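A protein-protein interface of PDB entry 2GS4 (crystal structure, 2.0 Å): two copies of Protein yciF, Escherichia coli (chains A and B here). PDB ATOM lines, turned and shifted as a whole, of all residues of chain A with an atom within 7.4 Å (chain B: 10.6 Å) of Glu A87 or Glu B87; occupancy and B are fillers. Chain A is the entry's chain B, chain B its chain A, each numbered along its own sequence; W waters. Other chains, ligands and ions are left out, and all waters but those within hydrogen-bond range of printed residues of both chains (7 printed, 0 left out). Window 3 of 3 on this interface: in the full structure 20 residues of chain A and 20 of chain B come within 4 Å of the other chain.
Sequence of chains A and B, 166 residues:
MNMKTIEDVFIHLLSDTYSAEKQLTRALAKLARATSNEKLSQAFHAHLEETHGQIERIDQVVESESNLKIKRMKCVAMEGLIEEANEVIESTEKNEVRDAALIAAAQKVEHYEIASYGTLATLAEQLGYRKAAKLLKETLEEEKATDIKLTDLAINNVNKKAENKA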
ATOM      1  N   LYS A  30       3.657   1.416 -14.702  1.00  0.00           N
ATOM      2  CA  LYS A  30       3.507   0.572 -13.519  1.00  0.00           C
ATOM      3  C   LYS A  30       4.388  -0.694 -13.588  1.00  0.00           C
ATOM      4  O   LYS A  30       4.990  -1.070 -12.591  1.00  0.00           O
ATOM      5  CB  LYS A  30       2.023   0.205 -13.332  1.00  0.00           C
ATOM      6  CG  LYS A  30       1.700  -0.786 -12.199  1.00  0.00           C
ATOM      7  CD  LYS A  30       0.182  -1.118 -12.169  1.00  0.00           C
ATOM      8  CE  LYS A  30      -0.154  -2.261 -11.201  1.00  0.00           C
ATOM      9  NZ  LYS A  30      -1.625  -2.538 -11.120  1.00  0.00           N
ATOM     10  N   GLY A  80      -8.244  -6.389 -20.416  1.00  0.00           N
ATOM     11  CA  GLY A  80      -8.026  -7.755 -19.975  1.00  0.00           C
ATOM     12  C   GLY A  80      -6.568  -8.186 -19.972  1.00  0.00           C
ATOM     13  O   GLY A  80      -6.112  -8.839 -19.025  1.00  0.00           O
ATOM     14  N   ILE A  82      -3.957  -6.212 -19.771  1.00  0.00           N
ATOM     15  CA  ILE A  82      -3.254  -5.451 -18.750  1.00  0.00           C
ATOM     16  C   ILE A  82      -3.559  -6.088 -17.379  1.00  0.00           C
ATOM     17  O   ILE A  82      -2.702  -6.109 -16.492  1.00  0.00           O
ATOM     18  CB  ILE A  82      -3.669  -3.940 -18.786  1.00  0.00           C
ATOM     19  CG1 ILE A  82      -2.889  -3.219 -19.904  1.00  0.00           C
ATOM     20  CG2 ILE A  82      -3.407  -3.281 -17.424  1.00  0.00           C
ATOM     21  CD1 ILE A  82      -3.325  -1.769 -20.197  1.00  0.00           C
ATOM     22  N   GLU A  83      -4.761  -6.639 -17.212  1.00  0.00           N
ATOM     23  CA  GLU A  83      -5.124  -7.253 -15.930  1.00  0.00           C
ATOM     24  C   GLU A  83      -4.335  -8.523 -15.618  1.00  0.00           C
ATOM     25  O   GLU A  83      -4.121  -8.848 -14.449  1.00  0.00           O
ATOM     26  CB  GLU A  83      -6.622  -7.568 -15.857  1.00  0.00           C
ATOM     27  CG  GLU A  83      -7.044  -8.032 -14.465  1.00  0.00           C
ATOM     28  CD  GLU A  83      -8.537  -8.238 -14.312  1.00  0.00           C
ATOM     29  OE1 GLU A  83      -8.969  -8.547 -13.180  1.00  0.00           O
ATOM     30  OE2 GLU A  83      -9.272  -8.090 -15.310  1.00  0.00           O
ATOM     31  N   GLU A  84      -3.903  -9.240 -16.651  1.00  0.00           N
ATOM     32  CA  GLU A  84      -3.125 -10.455 -16.430  1.00  0.00           C
ATOM     33  C   GLU A  84      -1.820 -10.083 -15.729  1.00  0.00           C
ATOM     34  O   GLU A  84      -1.378 -10.784 -14.822  1.00  0.00           O
ATOM     35  CB  GLU A  84      -2.853 -11.179 -17.759  1.00  0.00           C
ATOM     36  CG  GLU A  84      -4.125 -11.590 -18.484  1.00  0.00           C
ATOM     37  CD  GLU A  84      -3.877 -12.391 -19.752  1.00  0.00           C
ATOM     38  OE1 GLU A  84      -4.814 -12.481 -20.573  1.00  0.00           O
ATOM     39  OE2 GLU A  84      -2.764 -12.936 -19.926  1.00  0.00           O
ATOM     40  N   ALA A  85      -1.213  -8.973 -16.137  1.00  0.00           N
ATOM     41  CA  ALA A  85       0.021  -8.526 -15.510  1.00  0.00           C
ATOM     42  C   ALA A  85      -0.245  -8.125 -14.060  1.00  0.00           C
ATOM     43  O   ALA A  85       0.570  -8.407 -13.180  1.00  0.00           O
ATOM     44  CB  ALA A  85       0.615  -7.354 -16.294  1.00  0.00           C
ATOM     45  N   ASN A  86      -1.379  -7.465 -13.818  1.00  0.00           N
ATOM     46  CA  ASN A  86      -1.759  -7.049 -12.472  1.00  0.00           C
ATOM     47  C   ASN A  86      -1.861  -8.278 -11.567  1.00  0.00           C
ATOM     48  O   ASN A  86      -1.359  -8.277 -10.440  1.00  0.00           O
ATOM     49  CB  ASN A  86      -3.122  -6.339 -12.483  1.00  0.00           C
ATOM     50  CG  ASN A  86      -3.040  -4.886 -12.916  1.00  0.00           C
ATOM     51  OD1 ASN A  86      -4.074  -4.214 -13.062  1.00  0.00           O
ATOM     52  ND2 ASN A  86      -1.825  -4.388 -13.124  1.00  0.00           N
ATOM     53  N   GLU A  87      -2.523  -9.321 -12.066  1.00  0.00           N
ATOM     54  CA  GLU A  87      -2.697 -10.557 -11.314  1.00  0.00           C
ATOM     55  C   GLU A  87      -1.356 -11.225 -11.019  1.00  0.00           C
ATOM     56  O   GLU A  87      -1.178 -11.818  -9.949  1.00  0.00           O
ATOM     57  CB  GLU A  87      -3.606 -11.511 -12.088  1.00  0.00           C
ATOM     58  CG  GLU A  87      -3.698 -12.937 -11.518  1.00  0.00           C
ATOM     59  CD  GLU A  87      -4.410 -13.007 -10.179  1.00  0.00           C
ATOM     60  OE1 GLU A  87      -4.920 -11.968  -9.704  1.00  0.00           O
ATOM     61  OE2 GLU A  87      -4.460 -14.114  -9.608  1.00  0.00           O
ATOM     62  N   VAL A  88      -0.418 -11.135 -11.961  1.00  0.00           N
ATOM     63  CA  VAL A  88       0.904 -11.714 -11.742  1.00  0.00           C
ATOM     64  C   VAL A  88       1.536 -10.982 -10.558  1.00  0.00           C
ATOM     65  O   VAL A  88       2.053 -11.612  -9.632  1.00  0.00           O
ATOM     66  CB  VAL A  88       1.829 -11.540 -12.972  1.00  0.00           C
ATOM     67  CG1 VAL A  88       3.287 -11.721 -12.558  1.00  0.00           C
ATOM     68  CG2 VAL A  88       1.482 -12.555 -14.045  1.00  0.00           C
ATOM     69  N   ILE A  89       1.485  -9.651 -10.592  1.00  0.00           N
ATOM     70  CA  ILE A  89       2.057  -8.836  -9.524  1.00  0.00           C
ATOM     71  C   ILE A  89       1.484  -9.204  -8.158  1.00  0.00           C
ATOM     72  O   ILE A  89       2.222  -9.292  -7.169  1.00  0.00           O
ATOM     73  CB  ILE A  89       1.835  -7.317  -9.794  1.00  0.00           C
ATOM     74  CG1 ILE A  89       2.716  -6.862 -10.964  1.00  0.00           C
ATOM     75  CG2 ILE A  89       2.177  -6.503  -8.547  1.00  0.00           C
ATOM     76  CD1 ILE A  89       2.349  -5.498 -11.537  1.00  0.00           C
ATOM     77  N   GLU A  90       0.176  -9.435  -8.107  1.00  0.00           N
ATOM     78  CA  GLU A  90      -0.487  -9.780  -6.856  1.00  0.00           C
ATOM     79  C   GLU A  90      -0.255 -11.205  -6.361  1.00  0.00           C
ATOM     80  O   GLU A  90      -0.569 -11.530  -5.214  1.00  0.00           O
ATOM     81  CB  GLU A  90      -1.985  -9.533  -6.996  1.00  0.00           C
ATOM     82  CG  GLU A  90      -2.333  -8.059  -7.155  1.00  0.00           C
ATOM     83  CD  GLU A  90      -3.760  -7.857  -7.600  1.00  0.00           C
ATOM     84  OE1 GLU A  90      -4.353  -6.833  -7.215  1.00  0.00           O
ATOM     85  OE2 GLU A  90      -4.287  -8.714  -8.342  1.00  0.00           O
ATOM     86  N   SER A  91       0.297 -12.055  -7.216  1.00  0.00           N
ATOM     87  CA  SER A  91       0.541 -13.444  -6.831  1.00  0.00           C
ATOM     88  C   SER A  91       2.015 -13.838  -6.854  1.00  0.00           C
ATOM     89  O   SER A  91       2.345 -15.026  -6.977  1.00  0.00           O
ATOM     90  CB  SER A  91      -0.262 -14.392  -7.736  1.00  0.00           C
ATOM     91  OG  SER A  91       0.030 -14.153  -9.102  1.00  0.00           O
ATOM     92  N   THR A  92       2.904 -12.854  -6.734  1.00  0.00           N
ATOM     93  CA  THR A  92       4.336 -13.129  -6.729  1.00  0.00           C
ATOM     94  C   THR A  92       5.068 -12.115  -5.856  1.00  0.00           C
ATOM     95  O   THR A  92       4.571 -11.011  -5.626  1.00  0.00           O
ATOM     96  CB  THR A  92       4.949 -13.024  -8.150  1.00  0.00           C
ATOM     97  OG1 THR A  92       4.814 -11.678  -8.630  1.00  0.00           O
ATOM     98  CG2 THR A  92       4.252 -13.970  -9.114  1.00  0.00           C
ATOM     99  N   LEU A 102       5.733 -11.763 -15.797  1.00  0.00           N
ATOM    100  CA  LEU A 102       5.414 -10.480 -16.417  1.00  0.00           C
ATOM    101  C   LEU A 102       5.853 -10.511 -17.882  1.00  0.00           C
ATOM    102  O   LEU A 102       5.193  -9.934 -18.744  1.00  0.00           O
ATOM    103  CB  LEU A 102       6.099  -9.316 -15.681  1.00  0.00           C
ATOM    104  CG  LEU A 102       5.542  -8.926 -14.308  1.00  0.00           C
ATOM    105  CD1 LEU A 102       6.347  -7.749 -13.751  1.00  0.00           C
ATOM    106  CD2 LEU A 102       4.079  -8.542 -14.418  1.00  0.00           C
ATOM    107  N   ALA B  27     -16.122 -20.819 -20.614  1.00  0.00           N
ATOM    108  CA  ALA B  27     -16.289 -19.714 -19.677  1.00  0.00           C
ATOM    109  C   ALA B  27     -17.724 -19.494 -19.203  1.00  0.00           C
ATOM    110  O   ALA B  27     -17.962 -19.253 -18.022  1.00  0.00           O
ATOM    111  CB  ALA B  27     -15.747 -18.433 -20.288  1.00  0.00           C
ATOM    112  N   LYS B  30     -18.901 -21.972 -16.587  1.00  0.00           N
ATOM    113  CA  LYS B  30     -18.318 -21.638 -15.292  1.00  0.00           C
ATOM    114  C   LYS B  30     -19.058 -20.427 -14.715  1.00  0.00           C
ATOM    115  O   LYS B  30     -19.401 -20.413 -13.533  1.00  0.00           O
ATOM    116  CB  LYS B  30     -16.820 -21.310 -15.409  1.00  0.00           C
ATOM    117  CG  LYS B  30     -15.858 -22.494 -15.644  1.00  0.00           C
ATOM    118  CD  LYS B  30     -14.402 -22.056 -15.352  1.00  0.00           C
ATOM    119  CE  LYS B  30     -13.357 -23.127 -15.691  1.00  0.00           C
ATOM    120  NZ  LYS B  30     -11.981 -22.782 -15.188  1.00  0.00           N
ATOM    121  N   LEU B  31     -19.315 -19.413 -15.536  1.00  0.00           N
ATOM    122  CA  LEU B  31     -20.017 -18.238 -15.027  1.00  0.00           C
ATOM    123  C   LEU B  31     -21.394 -18.584 -14.496  1.00  0.00           C
ATOM    124  O   LEU B  31     -21.807 -18.064 -13.461  1.00  0.00           O
ATOM    125  CB  LEU B  31     -20.155 -17.159 -16.101  1.00  0.00           C
ATOM    126  CG  LEU B  31     -18.909 -16.343 -16.422  1.00  0.00           C
ATOM    127  CD1 LEU B  31     -19.173 -15.555 -17.685  1.00  0.00           C
ATOM    128  CD2 LEU B  31     -18.560 -15.415 -15.257  1.00  0.00           C
ATOM    129  N   ALA B  34     -21.035 -19.654 -11.115  1.00  0.00           N
ATOM    130  CA  ALA B  34     -20.341 -18.730 -10.221  1.00  0.00           C
ATOM    131  C   ALA B  34     -21.241 -17.800  -9.415  1.00  0.00           C
ATOM    132  O   ALA B  34     -20.749 -17.038  -8.579  1.00  0.00           O
ATOM    133  CB  ALA B  34     -19.337 -17.902 -11.023  1.00  0.00           C
ATOM    134  N   GLU B  79      -9.157 -14.681 -24.373  1.00  0.00           N
ATOM    135  CA  GLU B  79      -8.496 -15.367 -23.270  1.00  0.00           C
ATOM    136  C   GLU B  79      -8.350 -14.385 -22.099  1.00  0.00           C
ATOM    137  O   GLU B  79      -8.637 -14.729 -20.949  1.00  0.00           O
ATOM    138  CB  GLU B  79      -7.129 -15.880 -23.754  1.00  0.00           C
ATOM    139  CG  GLU B  79      -6.275 -16.640 -22.767  1.00  0.00           C
ATOM    140  CD  GLU B  79      -4.938 -17.043 -23.388  1.00  0.00           C
ATOM    141  OE1 GLU B  79      -4.730 -18.247 -23.652  1.00  0.00           O
ATOM    142  OE2 GLU B  79      -4.098 -16.148 -23.626  1.00  0.00           O
ATOM    143  N   GLY B  80      -7.929 -13.160 -22.401  1.00  0.00           N
ATOM    144  CA  GLY B  80      -7.774 -12.164 -21.355  1.00  0.00           C
ATOM    145  C   GLY B  80      -9.107 -11.769 -20.735  1.00  0.00           C
ATOM    146  O   GLY B  80      -9.209 -11.615 -19.517  1.00  0.00           O
ATOM    147  N   LEU B  81     -10.136 -11.614 -21.567  1.00  0.00           N
ATOM    148  CA  LEU B  81     -11.457 -11.227 -21.082  1.00  0.00           C
ATOM    149  C   LEU B  81     -12.050 -12.318 -20.192  1.00  0.00           C
ATOM    150  O   LEU B  81     -12.780 -12.032 -19.234  1.00  0.00           O
ATOM    151  CB  LEU B  81     -12.383 -10.931 -22.271  1.00  0.00           C
ATOM    152  CG  LEU B  81     -11.954  -9.707 -23.091  1.00  0.00           C
ATOM    153  CD1 LEU B  81     -12.831  -9.537 -24.334  1.00  0.00           C
ATOM    154  CD2 LEU B  81     -12.035  -8.474 -22.212  1.00  0.00           C
ATOM    155  N   ILE B  82     -11.719 -13.566 -20.509  1.00  0.00           N
ATOM    156  CA  ILE B  82     -12.204 -14.693 -19.738  1.00  0.00           C
ATOM    157  C   ILE B  82     -11.425 -14.766 -18.417  1.00  0.00           C
ATOM    158  O   ILE B  82     -11.994 -15.081 -17.373  1.00  0.00           O
ATOM    159  CB  ILE B  82     -12.117 -15.981 -20.595  1.00  0.00           C
ATOM    160  CG1 ILE B  82     -13.283 -15.964 -21.597  1.00  0.00           C
ATOM    161  CG2 ILE B  82     -12.123 -17.227 -19.721  1.00  0.00           C
ATOM    162  CD1 ILE B  82     -13.267 -17.042 -22.661  1.00  0.00           C
ATOM    163  N   GLU B  83     -10.136 -14.430 -18.437  1.00  0.00           N
ATOM    164  CA  GLU B  83      -9.369 -14.444 -17.193  1.00  0.00           C
ATOM    165  C   GLU B  83      -9.885 -13.317 -16.301  1.00  0.00           C
ATOM    166  O   GLU B  83      -9.877 -13.434 -15.075  1.00  0.00           O
ATOM    167  CB  GLU B  83      -7.862 -14.297 -17.470  1.00  0.00           C
ATOM    168  CG  GLU B  83      -7.257 -15.578 -18.046  1.00  0.00           C
ATOM    169  CD  GLU B  83      -5.799 -15.445 -18.431  1.00  0.00           C
ATOM    170  OE1 GLU B  83      -5.409 -16.056 -19.448  1.00  0.00           O
ATOM    171  OE2 GLU B  83      -5.042 -14.749 -17.720  1.00  0.00           O
ATOM    172  N   GLU B  84     -10.354 -12.233 -16.921  1.00  0.00           N
ATOM    173  CA  GLU B  84     -10.900 -11.096 -16.189  1.00  0.00           C
ATOM    174  C   GLU B  84     -12.133 -11.562 -15.417  1.00  0.00           C
ATOM    175  O   GLU B  84     -12.268 -11.294 -14.223  1.00  0.00           O
ATOM    176  CB  GLU B  84     -11.260  -9.953 -17.159  1.00  0.00           C
ATOM    177  CG  GLU B  84     -11.989  -8.770 -16.520  1.00  0.00           C
ATOM    178  CD  GLU B  84     -11.868  -7.489 -17.338  1.00  0.00           C
ATOM    179  OE1 GLU B  84     -11.659  -7.578 -18.568  1.00  0.00           O
ATOM    180  OE2 GLU B  84     -11.995  -6.389 -16.756  1.00  0.00           O
ATOM    181  N   ALA B  85     -13.022 -12.271 -16.101  1.00  0.00           N
ATOM    182  CA  ALA B  85     -14.225 -12.778 -15.464  1.00  0.00           C
ATOM    183  C   ALA B  85     -13.868 -13.791 -14.380  1.00  0.00           C
ATOM    184  O   ALA B  85     -14.456 -13.786 -13.302  1.00  0.00           O
ATOM    185  CB  ALA B  85     -15.133 -13.421 -16.509  1.00  0.00           C
ATOM    186  N   ASN B  86     -12.898 -14.657 -14.669  1.00  0.00           N
ATOM    187  CA  ASN B  86     -12.493 -15.678 -13.711  1.00  0.00           C
ATOM    188  C   ASN B  86     -11.920 -15.051 -12.442  1.00  0.00           C
ATOM    189  O   ASN B  86     -12.089 -15.593 -11.348  1.00  0.00           O
ATOM    190  CB  ASN B  86     -11.472 -16.634 -14.345  1.00  0.00           C
ATOM    191  CG  ASN B  86     -11.360 -17.948 -13.593  1.00  0.00           C
ATOM    192  OD1 ASN B  86     -12.366 -18.541 -13.185  1.00  0.00           O
ATOM    193  ND2 ASN B  86     -10.130 -18.422 -13.417  1.00  0.00           N
ATOM    194  N   GLU B  87     -11.238 -13.917 -12.577  1.00  0.00           N
ATOM    195  CA  GLU B  87     -10.681 -13.259 -11.403  1.00  0.00           C
ATOM    196  C   GLU B  87     -11.816 -12.862 -10.460  1.00  0.00           C
ATOM    197  O   GLU B  87     -11.634 -12.803  -9.249  1.00  0.00           O
ATOM    198  CB  GLU B  87      -9.870 -12.027 -11.798  1.00  0.00           C
ATOM    199  CG  GLU B  87      -8.379 -12.206 -11.630  1.00  0.00           C
ATOM    200  CD  GLU B  87      -7.638 -10.894 -11.676  1.00  0.00           C
ATOM    201  OE1 GLU B  87      -7.778 -10.099 -10.723  1.00  0.00           O
ATOM    202  OE2 GLU B  87      -6.923 -10.651 -12.667  1.00  0.00           O
ATOM    203  N   VAL B  88     -12.991 -12.578 -11.024  1.00  0.00           N
ATOM    204  CA  VAL B  88     -14.152 -12.221 -10.205  1.00  0.00           C
ATOM    205  C   VAL B  88     -14.706 -13.503  -9.587  1.00  0.00           C
ATOM    206  O   VAL B  88     -14.967 -13.558  -8.384  1.00  0.00           O
ATOM    207  CB  VAL B  88     -15.274 -11.534 -11.039  1.00  0.00           C
ATOM    208  CG1 VAL B  88     -16.505 -11.320 -10.182  1.00  0.00           C
ATOM    209  CG2 VAL B  88     -14.776 -10.177 -11.572  1.00  0.00           C
ATOM    210  N   ILE B  89     -14.871 -14.526 -10.424  1.00  0.00           N
ATOM    211  CA  ILE B  89     -15.385 -15.840 -10.005  1.00  0.00           C
ATOM    212  C   ILE B  89     -14.590 -16.404  -8.828  1.00  0.00           C
ATOM    213  O   ILE B  89     -15.159 -16.883  -7.840  1.00  0.00           O
ATOM    214  CB  ILE B  89     -15.287 -16.898 -11.165  1.00  0.00           C
ATOM    215  CG1 ILE B  89     -16.274 -16.569 -12.289  1.00  0.00           C
ATOM    216  CG2 ILE B  89     -15.533 -18.305 -10.621  1.00  0.00           C
ATOM    217  CD1 ILE B  89     -16.037 -17.362 -13.586  1.00  0.00           C
ATOM    218  N   GLU B  90     -13.269 -16.339  -8.944  1.00  0.00           N
ATOM    219  CA  GLU B  90     -12.370 -16.876  -7.933  1.00  0.00           C
ATOM    220  C   GLU B  90     -12.053 -15.959  -6.751  1.00  0.00           C
ATOM    221  O   GLU B  90     -11.265 -16.329  -5.874  1.00  0.00           O
ATOM    222  CB  GLU B  90     -11.068 -17.302  -8.615  1.00  0.00           C
ATOM    223  CG  GLU B  90     -11.267 -18.264  -9.783  1.00  0.00           C
ATOM    224  CD  GLU B  90     -11.554 -19.685  -9.329  1.00  0.00           C
ATOM    225  OE1 GLU B  90     -10.686 -20.286  -8.659  1.00  0.00           O
ATOM    226  OE2 GLU B  90     -12.648 -20.198  -9.643  1.00  0.00           O
ATOM    227  N   SER B  91     -12.645 -14.766  -6.726  1.00  0.00           N
ATOM    228  CA  SER B  91     -12.402 -13.832  -5.626  1.00  0.00           C
ATOM    229  C   SER B  91     -13.362 -14.165  -4.490  1.00  0.00           C
ATOM    230  O   SER B  91     -14.150 -15.107  -4.600  1.00  0.00           O
ATOM    231  CB  SER B  91     -12.681 -12.404  -6.075  1.00  0.00           C
ATOM    232  OG  SER B  91     -14.081 -12.200  -6.200  1.00  0.00           O
ATOM    233  N   THR B  92     -13.296 -13.404  -3.398  1.00  0.00           N
ATOM    234  CA  THR B  92     -14.225 -13.642  -2.298  1.00  0.00           C
ATOM    235  C   THR B  92     -15.378 -12.649  -2.365  1.00  0.00           C
ATOM    236  O   THR B  92     -16.141 -12.528  -1.410  1.00  0.00           O
ATOM    237  CB  THR B  92     -13.570 -13.541  -0.882  1.00  0.00           C
ATOM    238  OG1 THR B  92     -12.853 -12.311  -0.756  1.00  0.00           O
ATOM    239  CG2 THR B  92     -12.632 -14.714  -0.634  1.00  0.00           C
ATOM    240  N   GLU B  93     -15.501 -11.923  -3.479  1.00  0.00           N
ATOM    241  CA  GLU B  93     -16.605 -10.977  -3.620  1.00  0.00           C
ATOM    242  C   GLU B  93     -17.842 -11.826  -3.403  1.00  0.00           C
ATOM    243  O   GLU B  93     -17.842 -13.015  -3.707  1.00  0.00           O
ATOM    244  CB  GLU B  93     -16.638 -10.335  -5.013  1.00  0.00           C
ATOM    245  CG  GLU B  93     -15.481  -9.387  -5.296  1.00  0.00           C
ATOM    246  CD  GLU B  93     -15.571  -8.753  -6.671  1.00  0.00           C
ATOM    247  OE1 GLU B  93     -14.507  -8.484  -7.268  1.00  0.00           O
ATOM    248  OE2 GLU B  93     -16.702  -8.514  -7.153  1.00  0.00           O
ATOM    249  N   LYS B  94     -18.900 -11.226  -2.881  1.00  0.00           N
ATOM    250  CA  LYS B  94     -20.097 -12.000  -2.599  1.00  0.00           C
ATOM    251  C   LYS B  94     -21.379 -11.249  -2.952  1.00  0.00           C
ATOM    252  O   LYS B  94     -21.400 -10.015  -3.012  1.00  0.00           O
ATOM    253  CB  LYS B  94     -20.058 -12.418  -1.120  1.00  0.00           C
ATOM    254  CG  LYS B  94     -21.071 -13.452  -0.678  1.00  0.00           C
ATOM    255  CD  LYS B  94     -20.815 -13.852   0.783  1.00  0.00           C
ATOM    256  CE  LYS B  94     -19.656 -14.842   0.911  1.00  0.00           C
ATOM    257  NZ  LYS B  94     -18.970 -14.812   2.248  1.00  0.00           N
ATOM    258  N   VAL B  97     -22.145  -7.556  -4.699  1.00  0.00           N
ATOM    259  CA  VAL B  97     -20.840  -7.057  -5.141  1.00  0.00           C
ATOM    260  C   VAL B  97     -20.384  -7.993  -6.241  1.00  0.00           C
ATOM    261  O   VAL B  97     -20.048  -7.579  -7.354  1.00  0.00           O
ATOM    262  CB  VAL B  97     -19.804  -7.112  -4.002  1.00  0.00           C
ATOM    263  CG1 VAL B  97     -18.509  -6.469  -4.428  1.00  0.00           C
ATOM    264  CG2 VAL B  97     -20.370  -6.433  -2.770  1.00  0.00           C
ATOM    265  N   ARG B  98     -20.390  -9.272  -5.899  1.00  0.00           N
ATOM    266  CA  ARG B  98     -19.998 -10.334  -6.796  1.00  0.00           C
ATOM    267  C   ARG B  98     -20.746 -10.302  -8.122  1.00  0.00           C
ATOM    268  O   ARG B  98     -20.136 -10.387  -9.190  1.00  0.00           O
ATOM    269  CB  ARG B  98     -20.231 -11.675  -6.108  1.00  0.00           C
ATOM    270  CG  ARG B  98     -19.924 -12.857  -6.979  1.00  0.00           C
ATOM    271  CD  ARG B  98     -19.951 -14.145  -6.183  1.00  0.00           C
ATOM    272  NE  ARG B  98     -19.364 -15.233  -6.955  1.00  0.00           N
ATOM    273  CZ  ARG B  98     -18.100 -15.628  -6.855  1.00  0.00           C
ATOM    274  NH1 ARG B  98     -17.654 -16.621  -7.610  1.00  0.00           N
ATOM    275  NH2 ARG B  98     -17.283 -15.045  -5.984  1.00  0.00           N
ATOM    276  N   ALA B 101     -19.927  -7.310 -10.524  1.00  0.00           N
ATOM    277  CA  ALA B 101     -18.677  -7.563 -11.224  1.00  0.00           C
ATOM    278  C   ALA B 101     -18.857  -8.623 -12.311  1.00  0.00           C
ATOM    279  O   ALA B 101     -18.322  -8.485 -13.404  1.00  0.00           O
ATOM    280  CB  ALA B 101     -17.608  -8.006 -10.234  1.00  0.00           C
ATOM    281  N   LEU B 102     -19.612  -9.673 -12.017  1.00  0.00           N
ATOM    282  CA  LEU B 102     -19.826 -10.732 -13.006  1.00  0.00           C
ATOM    283  C   LEU B 102     -20.563 -10.195 -14.229  1.00  0.00           C
ATOM    284  O   LEU B 102     -20.182 -10.465 -15.367  1.00  0.00           O
ATOM    285  CB  LEU B 102     -20.588 -11.907 -12.380  1.00  0.00           C
ATOM    286  CG  LEU B 102     -19.747 -12.688 -11.362  1.00  0.00           C
ATOM    287  CD1 LEU B 102     -20.598 -13.746 -10.662  1.00  0.00           C
ATOM    288  CD2 LEU B 102     -18.570 -13.336 -12.069  1.00  0.00           C
ATOM    289  N   ALA B 105     -18.201  -7.889 -16.085  1.00  0.00           N
ATOM    290  CA  ALA B 105     -17.199  -8.646 -16.820  1.00  0.00           C
ATOM    291  C   ALA B 105     -17.845  -9.210 -18.080  1.00  0.00           C
ATOM    292  O   ALA B 105     -17.253  -9.179 -19.154  1.00  0.00           O
ATOM    293  CB  ALA B 105     -16.643  -9.769 -15.953  1.00  0.00           C
ATOM    294  N   ALA B 106     -19.065  -9.718 -17.944  1.00  0.00           N
ATOM    295  CA  ALA B 106     -19.788 -10.282 -19.080  1.00  0.00           C
ATOM    296  C   ALA B 106     -20.101  -9.221 -20.132  1.00  0.00           C
ATOM    297  O   ALA B 106     -20.144  -9.520 -21.327  1.00  0.00           O
ATOM    298  CB  ALA B 106     -21.080 -10.956 -18.608  1.00  0.00           C
HETATM  299  O   HOH W   1     -11.540  -9.015 -13.027  1.00  0.00           O
HETATM  300  O   HOH W   2      -4.496 -13.633 -22.918  1.00  0.00           O
HETATM  301  O   HOH W   3      -7.460 -10.688 -17.648  1.00  0.00           O
HETATM  302  O   HOH W   4      -7.019 -11.459  -7.594  1.00  0.00           O
HETATM  303  O   HOH W   5      -2.492 -15.508 -19.925  1.00  0.00           O
HETATM  304  O   HOH W   6     -11.810  -6.064 -14.304  1.00  0.00           O
HETATM  305  O   HOH W   7      -6.419 -11.402 -15.056  1.00  0.00           O
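The side-chain carboxylate (OE1) of Glu A83 sits close to the side-chain carboxylate (OE2) of Glu B87 (3.0 Å).
The side-chain hydroxyl of Ser A91 is in hydrogen-bond range of the backbone carbonyl oxygen of Glu A87 (2.8 Å).
OE1 of Glu B84 touches CA of Gly A80, 3.9 Å away. Glu A83 touches Glu B84. Gly B80 touches Glu A84 (CA to OE1, 3.1 Å). OE2 of Glu B83 touches CD of Glu A84, 3.3 Å away. Glu B87 touches Glu A87.
Of chain A, only Glu A83 (3.0 Å) and Glu A87 (3.5 Å) come within 4 Å of Glu B87. Of chain B, only Glu B84 (3.1 Å) and Glu B87 (3.0 Å) come within 4 Å of Glu A83. No residue of chain B comes within 4 Å of Ala A85. No residue of chain B comes within 4 Å of Ile A89. No residue of chain B comes within 4 Å of Ser A91. Printed residues of chain A within 4 Å of Gly B80: Glu A84. Of the printed residues of chain B, Glu A84 touches Gly B80 (3.1 Å) and Glu B83 (3.3 Å). Of the printed residues of chain A, Glu B83 touches Glu A84. The nearest residue of chain B that does not touch Glu A87 is Glu B83 (6.6 Å). The nearest residue of chain A that does not touch Glu B87 is Glu A90 (4.4 Å).
Of the 26 printed residues of chain B, 4 touch a printed residue of chain A. Among the printed residues, no Asp or Glu carboxylate lies within 4 Å of a Lys or Arg side-chain nitrogen of the other chain.
Gly A80 touches Glu B84, and with the chains exchanged Glu A84 touches Gly B80. Glu A83 touches Glu B84, and with the chains exchanged Glu A84 touches Glu B83. Glu A83 touches Glu B87, but with the chains exchanged Glu A87 does not touch Glu B83 (6.6 Å). Glu B87 touches its own counterpart, Glu A87. Of the 6 pairs that touch across the chains among the printed residues, 5 have their exchanged pair printed and touching as well.
Water W6 lies within hydrogen-bond range of the side-chain carboxylate (OE2) of Glu B84 (2.5 Å) and the side-chain carboxylate (OE2) of Glu A83 (3.4 Å). Water W7 bridges OE2 of Glu B87 (2.6 Å) and O of Glu A83 (3.5 Å). Water W1 lies within hydrogen-bond range of the side-chain carboxylate of Glu A83 and the backbone carbonyl oxygen of Glu B84. Water W2 lies within hydrogen-bond range of OE1 of Glu A84 and OE2 of Glu B79. Water W3 lies within hydrogen-bond range of O of Gly A80 (2.7 Å), O of Gly B80 (2.7 Å) and N of Glu B84 (3.4 Å). Water W4 bridges OE1 of Glu A87 and OE1 of Glu B87.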
